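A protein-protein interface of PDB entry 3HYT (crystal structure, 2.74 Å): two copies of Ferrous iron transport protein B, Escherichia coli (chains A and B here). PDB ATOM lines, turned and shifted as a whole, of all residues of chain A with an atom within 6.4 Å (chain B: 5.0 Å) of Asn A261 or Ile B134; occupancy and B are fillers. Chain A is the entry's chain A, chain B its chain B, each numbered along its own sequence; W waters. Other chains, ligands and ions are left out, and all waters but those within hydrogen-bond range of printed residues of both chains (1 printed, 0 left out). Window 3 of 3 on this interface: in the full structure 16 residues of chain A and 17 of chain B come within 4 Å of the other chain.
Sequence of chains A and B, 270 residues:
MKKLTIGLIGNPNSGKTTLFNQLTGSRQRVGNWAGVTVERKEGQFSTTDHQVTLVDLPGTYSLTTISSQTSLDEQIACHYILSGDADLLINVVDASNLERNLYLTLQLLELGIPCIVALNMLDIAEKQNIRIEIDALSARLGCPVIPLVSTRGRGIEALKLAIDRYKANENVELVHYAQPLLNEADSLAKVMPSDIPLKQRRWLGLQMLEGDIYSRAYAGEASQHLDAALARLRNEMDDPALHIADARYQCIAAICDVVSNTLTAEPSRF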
ATOM      1  N   ASN A 129      12.034  -1.412  10.862  1.00  0.00           N
ATOM      2  CA  ASN A 129      12.678  -2.411   9.997  1.00  0.00           C
ATOM      3  C   ASN A 129      11.949  -2.638   8.659  1.00  0.00           C
ATOM      4  O   ASN A 129      12.074  -3.704   8.044  1.00  0.00           O
ATOM      5  CB  ASN A 129      12.895  -3.732  10.768  1.00  0.00           C
ATOM      6  CG  ASN A 129      13.688  -4.763   9.975  1.00  0.00           C
ATOM      7  OD1 ASN A 129      14.716  -4.451   9.366  1.00  0.00           O
ATOM      8  ND2 ASN A 129      13.212  -6.004   9.987  1.00  0.00           N
ATOM      9  N   ILE A 130      11.202  -1.625   8.217  1.00  0.00           N
ATOM     10  CA  ILE A 130      10.467  -1.674   6.950  1.00  0.00           C
ATOM     11  C   ILE A 130      11.296  -1.057   5.829  1.00  0.00           C
ATOM     12  O   ILE A 130      11.615   0.134   5.865  1.00  0.00           O
ATOM     13  CB  ILE A 130       9.087  -0.956   7.043  1.00  0.00           C
ATOM     14  CG1 ILE A 130       8.202  -1.621   8.105  1.00  0.00           C
ATOM     15  CG2 ILE A 130       8.379  -0.955   5.686  1.00  0.00           C
ATOM     16  CD1 ILE A 130       7.059  -0.746   8.612  1.00  0.00           C
ATOM     17  N   ARG A 131      11.639  -1.877   4.839  1.00  0.00           N
ATOM     18  CA  ARG A 131      12.405  -1.427   3.675  1.00  0.00           C
ATOM     19  C   ARG A 131      11.537  -1.383   2.409  1.00  0.00           C
ATOM     20  O   ARG A 131      10.856  -2.356   2.084  1.00  0.00           O
ATOM     21  CB  ARG A 131      13.624  -2.330   3.467  1.00  0.00           C
ATOM     22  N   ILE A 132      11.562  -0.250   1.709  1.00  0.00           N
ATOM     23  CA  ILE A 132      10.763  -0.045   0.494  1.00  0.00           C
ATOM     24  C   ILE A 132      11.652   0.095  -0.741  1.00  0.00           C
ATOM     25  O   ILE A 132      12.541   0.942  -0.778  1.00  0.00           O
ATOM     26  CB  ILE A 132       9.872   1.233   0.587  1.00  0.00           C
ATOM     27  CG1 ILE A 132       9.093   1.307   1.912  1.00  0.00           C
ATOM     28  CG2 ILE A 132       8.954   1.361  -0.637  1.00  0.00           C
ATOM     29  CD1 ILE A 132       7.906   0.366   2.036  1.00  0.00           C
ATOM     30  N   GLU A 133      11.395  -0.731  -1.752  1.00  0.00           N
ATOM     31  CA  GLU A 133      12.080  -0.623  -3.043  1.00  0.00           C
ATOM     32  C   GLU A 133      11.448   0.488  -3.907  1.00  0.00           C
ATOM     33  O   GLU A 133      10.433   0.276  -4.575  1.00  0.00           O
ATOM     34  CB  GLU A 133      12.067  -1.975  -3.768  1.00  0.00           C
ATOM     35  CG  GLU A 133      13.158  -2.137  -4.822  1.00  0.00           C
ATOM     36  CD  GLU A 133      13.236  -3.551  -5.391  1.00  0.00           C
ATOM     37  OE1 GLU A 133      12.987  -4.526  -4.642  1.00  0.00           O
ATOM     38  OE2 GLU A 133      13.559  -3.686  -6.594  1.00  0.00           O
ATOM     39  N   ARG A 140       5.302   0.500 -10.887  1.00  0.00           N
ATOM     40  CA  ARG A 140       3.948  -0.038 -10.806  1.00  0.00           C
ATOM     41  C   ARG A 140       2.890   1.049 -10.630  1.00  0.00           C
ATOM     42  O   ARG A 140       1.777   0.918 -11.137  1.00  0.00           O
ATOM     43  CB  ARG A 140       3.862  -1.073  -9.690  1.00  0.00           C
ATOM     44  CG  ARG A 140       4.498  -2.390 -10.065  1.00  0.00           C
ATOM     45  CD  ARG A 140       5.042  -3.124  -8.859  1.00  0.00           C
ATOM     46  NE  ARG A 140       5.667  -4.388  -9.253  1.00  0.00           N
ATOM     47  CZ  ARG A 140       6.921  -4.516  -9.685  1.00  0.00           C
ATOM     48  NH1 ARG A 140       7.721  -3.459  -9.784  1.00  0.00           N
ATOM     49  NH2 ARG A 140       7.378  -5.713 -10.018  1.00  0.00           N
ATOM     50  N   CYS A 256       2.695  -4.174  -2.503  1.00  0.00           N
ATOM     51  CA  CYS A 256       3.351  -4.412  -1.211  1.00  0.00           C
ATOM     52  C   CYS A 256       4.195  -5.680  -1.200  1.00  0.00           C
ATOM     53  O   CYS A 256       5.260  -5.718  -0.586  1.00  0.00           O
ATOM     54  CB  CYS A 256       2.308  -4.505  -0.095  1.00  0.00           C
ATOM     55  SG  CYS A 256       1.341  -3.008   0.157  1.00  0.00           S
ATOM     56  N   ASP A 257       3.703  -6.713  -1.881  1.00  0.00           N
ATOM     57  CA  ASP A 257       4.380  -8.003  -1.970  1.00  0.00           C
ATOM     58  C   ASP A 257       5.754  -7.895  -2.626  1.00  0.00           C
ATOM     59  O   ASP A 257       6.712  -8.511  -2.161  1.00  0.00           O
ATOM     60  CB  ASP A 257       3.518  -8.996  -2.752  1.00  0.00           C
ATOM     61  CG  ASP A 257       4.122 -10.384  -2.796  1.00  0.00           C
ATOM     62  OD1 ASP A 257       3.947 -11.143  -1.822  1.00  0.00           O
ATOM     63  OD2 ASP A 257       4.765 -10.721  -3.813  1.00  0.00           O
ATOM     64  N   VAL A 258       5.837  -7.119  -3.704  1.00  0.00           N
ATOM     65  CA  VAL A 258       7.074  -6.970  -4.465  1.00  0.00           C
ATOM     66  C   VAL A 258       7.933  -5.863  -3.875  1.00  0.00           C
ATOM     67  O   VAL A 258       9.147  -5.999  -3.753  1.00  0.00           O
ATOM     68  CB  VAL A 258       6.790  -6.650  -5.965  1.00  0.00           C
ATOM     69  CG1 VAL A 258       8.091  -6.414  -6.729  1.00  0.00           C
ATOM     70  CG2 VAL A 258       5.980  -7.758  -6.619  1.00  0.00           C
ATOM     71  N   VAL A 259       7.277  -4.777  -3.493  1.00  0.00           N
ATOM     72  CA  VAL A 259       7.932  -3.523  -3.137  1.00  0.00           C
ATOM     73  C   VAL A 259       8.460  -3.466  -1.693  1.00  0.00           C
ATOM     74  O   VAL A 259       9.504  -2.858  -1.438  1.00  0.00           O
ATOM     75  CB  VAL A 259       6.970  -2.341  -3.465  1.00  0.00           C
ATOM     76  CG1 VAL A 259       7.238  -1.109  -2.620  1.00  0.00           C
ATOM     77  CG2 VAL A 259       7.036  -2.027  -4.944  1.00  0.00           C
ATOM     78  N   SER A 260       7.759  -4.115  -0.763  1.00  0.00           N
ATOM     79  CA  SER A 260       8.075  -3.979   0.656  1.00  0.00           C
ATOM     80  C   SER A 260       8.285  -5.299   1.393  1.00  0.00           C
ATOM     81  O   SER A 260       7.324  -5.951   1.792  1.00  0.00           O
ATOM     82  CB  SER A 260       6.986  -3.168   1.355  1.00  0.00           C
ATOM     83  OG  SER A 260       7.353  -2.900   2.695  1.00  0.00           O
ATOM     84  N   ASN A 261       9.546  -5.674   1.592  1.00  0.00           N
ATOM     85  CA  ASN A 261       9.895  -6.895   2.331  1.00  0.00           C
ATOM     86  C   ASN A 261      10.928  -6.652   3.437  1.00  0.00           C
ATOM     87  O   ASN A 261      10.938  -5.602   4.087  1.00  0.00           O
ATOM     88  CB  ASN A 261      10.398  -7.988   1.375  1.00  0.00           C
ATOM     89  CG  ASN A 261       9.445  -8.238   0.208  1.00  0.00           C
ATOM     90  OD1 ASN A 261       8.243  -8.435   0.401  1.00  0.00           O
ATOM     91  ND2 ASN A 261       9.985  -8.238  -1.009  1.00  0.00           N
ATOM     92  N   LEU B 119       9.676 -16.400  -5.598  1.00  0.00           N
ATOM     93  CA  LEU B 119      10.619 -16.486  -4.489  1.00  0.00           C
ATOM     94  C   LEU B 119       9.943 -17.009  -3.234  1.00  0.00           C
ATOM     95  O   LEU B 119       9.060 -16.363  -2.669  1.00  0.00           O
ATOM     96  CB  LEU B 119      11.296 -15.140  -4.218  1.00  0.00           C
ATOM     97  CG  LEU B 119      12.476 -14.764  -5.118  1.00  0.00           C
ATOM     98  CD1 LEU B 119      13.050 -13.427  -4.691  1.00  0.00           C
ATOM     99  CD2 LEU B 119      13.560 -15.837  -5.109  1.00  0.00           C
ATOM    100  N   ILE B 132      17.415  -9.397  -1.322  1.00  0.00           N
ATOM    101  CA  ILE B 132      17.375  -9.510  -2.780  1.00  0.00           C
ATOM    102  C   ILE B 132      16.574  -8.355  -3.374  1.00  0.00           C
ATOM    103  O   ILE B 132      15.445  -8.100  -2.964  1.00  0.00           O
ATOM    104  CB  ILE B 132      16.756 -10.861  -3.232  1.00  0.00           C
ATOM    105  CG1 ILE B 132      17.682 -12.028  -2.876  1.00  0.00           C
ATOM    106  CG2 ILE B 132      16.473 -10.862  -4.729  1.00  0.00           C
ATOM    107  CD1 ILE B 132      17.013 -13.389  -2.935  1.00  0.00           C
ATOM    108  N   GLU B 133      17.171  -7.658  -4.335  1.00  0.00           N
ATOM    109  CA  GLU B 133      16.487  -6.580  -5.041  1.00  0.00           C
ATOM    110  C   GLU B 133      15.656  -7.178  -6.175  1.00  0.00           C
ATOM    111  O   GLU B 133      16.176  -7.483  -7.253  1.00  0.00           O
ATOM    112  CB  GLU B 133      17.507  -5.567  -5.561  1.00  0.00           C
ATOM    113  CG  GLU B 133      16.931  -4.207  -5.916  1.00  0.00           C
ATOM    114  CD  GLU B 133      18.013  -3.181  -6.213  1.00  0.00           C
ATOM    115  OE1 GLU B 133      18.048  -2.668  -7.354  1.00  0.00           O
ATOM    116  OE2 GLU B 133      18.834  -2.895  -5.309  1.00  0.00           O
ATOM    117  N   ILE B 134      14.362  -7.345  -5.908  1.00  0.00           N
ATOM    118  CA  ILE B 134      13.442  -8.097  -6.774  1.00  0.00           C
ATOM    119  C   ILE B 134      13.375  -7.601  -8.227  1.00  0.00           C
ATOM    120  O   ILE B 134      13.472  -8.401  -9.160  1.00  0.00           O
ATOM    121  CB  ILE B 134      12.012  -8.199  -6.145  1.00  0.00           C
ATOM    122  CG1 ILE B 134      11.985  -9.228  -5.014  1.00  0.00           C
ATOM    123  CG2 ILE B 134      10.976  -8.604  -7.178  1.00  0.00           C
ATOM    124  CD1 ILE B 134      12.216  -8.656  -3.639  1.00  0.00           C
ATOM    125  N   ASP B 135      13.216  -6.293  -8.415  1.00  0.00           N
ATOM    126  CA  ASP B 135      13.126  -5.719  -9.761  1.00  0.00           C
ATOM    127  C   ASP B 135      14.415  -5.830 -10.572  1.00  0.00           C
ATOM    128  O   ASP B 135      14.371  -5.954 -11.797  1.00  0.00           O
ATOM    129  CB  ASP B 135      12.650  -4.267  -9.711  1.00  0.00           C
ATOM    130  CG  ASP B 135      11.229  -4.102 -10.216  1.00  0.00           C
ATOM    131  OD1 ASP B 135      10.396  -5.008  -9.982  1.00  0.00           O
ATOM    132  OD2 ASP B 135      10.947  -3.063 -10.854  1.00  0.00           O
ATOM    133  N   ALA B 136      15.553  -5.777  -9.885  1.00  0.00           N
ATOM    134  CA  ALA B 136      16.852  -5.951 -10.523  1.00  0.00           C
ATOM    135  C   ALA B 136      17.002  -7.376 -11.054  1.00  0.00           C
ATOM    136  O   ALA B 136      17.578  -7.592 -12.121  1.00  0.00           O
ATOM    137  CB  ALA B 136      17.964  -5.623  -9.545  1.00  0.00           C
ATOM    138  N   LEU B 137      16.470  -8.336 -10.302  1.00  0.00           N
ATOM    139  CA  LEU B 137      16.463  -9.734 -10.708  1.00  0.00           C
ATOM    140  C   LEU B 137      15.531  -9.945 -11.899  1.00  0.00           C
ATOM    141  O   LEU B 137      15.899 -10.596 -12.882  1.00  0.00           O
ATOM    142  CB  LEU B 137      16.051 -10.630  -9.535  1.00  0.00           C
ATOM    143  CG  LEU B 137      16.060 -12.143  -9.754  1.00  0.00           C
ATOM    144  CD1 LEU B 137      17.457 -12.642 -10.067  1.00  0.00           C
ATOM    145  CD2 LEU B 137      15.499 -12.869  -8.544  1.00  0.00           C
ATOM    146  N   SER B 138      14.328  -9.383 -11.798  1.00  0.00           N
ATOM    147  CA  SER B 138      13.329  -9.469 -12.851  1.00  0.00           C
ATOM    148  C   SER B 138      13.893  -8.967 -14.172  1.00  0.00           C
ATOM    149  O   SER B 138      13.758  -9.627 -15.202  1.00  0.00           O
ATOM    150  CB  SER B 138      12.086  -8.666 -12.466  1.00  0.00           C
ATOM    151  OG  SER B 138      11.029  -8.904 -13.378  1.00  0.00           O
ATOM    152  N   VAL B 145       9.348 -11.528 -11.085  1.00  0.00           N
ATOM    153  CA  VAL B 145       9.823 -12.177  -9.869  1.00  0.00           C
ATOM    154  C   VAL B 145       8.836 -11.841  -8.755  1.00  0.00           C
ATOM    155  O   VAL B 145       8.629 -10.671  -8.436  1.00  0.00           O
ATOM    156  CB  VAL B 145      11.270 -11.740  -9.516  1.00  0.00           C
ATOM    157  CG1 VAL B 145      11.709 -12.309  -8.174  1.00  0.00           C
ATOM    158  CG2 VAL B 145      12.233 -12.179 -10.610  1.00  0.00           C
ATOM    159  N   PRO B 147       7.676 -12.541  -4.846  1.00  0.00           N
ATOM    160  CA  PRO B 147       7.915 -13.090  -3.510  1.00  0.00           C
ATOM    161  C   PRO B 147       6.657 -13.753  -2.956  1.00  0.00           C
ATOM    162  O   PRO B 147       5.555 -13.240  -3.151  1.00  0.00           O
ATOM    163  CB  PRO B 147       8.274 -11.856  -2.678  1.00  0.00           C
ATOM    164  CG  PRO B 147       8.687 -10.823  -3.670  1.00  0.00           C
ATOM    165  CD  PRO B 147       7.851 -11.078  -4.879  1.00  0.00           C
ATOM    166  N   VAL B 149       5.032 -13.962  -0.005  1.00  0.00           N
ATOM    167  CA  VAL B 149       4.692 -13.470   1.333  1.00  0.00           C
ATOM    168  C   VAL B 149       3.350 -14.070   1.747  1.00  0.00           C
ATOM    169  O   VAL B 149       2.384 -14.040   0.983  1.00  0.00           O
ATOM    170  CB  VAL B 149       4.623 -11.915   1.381  1.00  0.00           C
ATOM    171  CG1 VAL B 149       4.291 -11.420   2.780  1.00  0.00           C
ATOM    172  CG2 VAL B 149       5.930 -11.297   0.896  1.00  0.00           C
HETATM  173  O   HOH W   1      15.566  -1.765  -7.865  1.00  0.00           O
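The side-chain carboxylate (OD2) of Asp A257 lies close to the backbone carbonyl oxygen (O) of Pro B147 (2.7 Å).
The side-chain carboxylate (OE1) of Glu A133 lies within hydrogen-bond range of the backbone NH (N) of Ile B134, at 3.4 Å.
N of Asp B135 sits at hydrogen-bond distance from OE2 of Glu A133 (3.2 Å).
NH1 of Arg A140 lies within salt-bridge range of OD1 of Asp B135, at 3.1 Å.
OD1 of Asn A261 sits close to O of Asp A257, at 3.0 Å.
The backbone NH (N) of Glu A133 is in hydrogen-bond range of the backbone carbonyl oxygen (O) of Val A259, at 2.9 Å.
Among the printed residues, pairs that only touch across the chains: Asp A257 with Val B149 (3.4 Å), Asn A261 with Ile B134 (3.5 Å), Glu A133 with Glu B133 (3.5 Å), Val A258 with Ile B134 (3.6 Å), Asn A261 with Val B149 (3.7 Å) and Asn A261 with Pro B147 (3.9 Å).
Printed residues of chain B within 4 Å of Asp A257: Pro B147 and Val B149.
Asn A261 touches just these residues of chain B: Ile B134, Pro B147 and Val B149.
Leu B119 touches none of the printed residues of chain A.
Of the printed residues of chain A, Pro B147 touches Asp A257 (2.7 Å) and Asn A261 (3.9 Å).
Printed residues of chain A within 4 Å of Val B149: Asp A257 (3.4 Å) and Asn A261 (3.7 Å).
The nearest residue of chain A that does not touch Ile B134 is Arg A140 (5.4 Å).
The nearest printed residue of chain A that does not touch Val B149 is Ser A260 (5.6 Å).
Hydrophobic or aromatic side chains of chain A within 4 Å of the printed part of chain B: Val A258.
Along chain A the printed residues that touch a printed residue of chain B span positions 133 to 261.
Among the printed residues, 10 pairs touch across the chains.
Glu A133 touches its own counterpart, Glu B133.
2 positions are printed for both chains.
Water W1 bridges the side-chain carboxylate (OE1) of Glu B133 (2.7 Å) and the side-chain carboxylate (OE2) of Glu A133 (3.1 Å).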
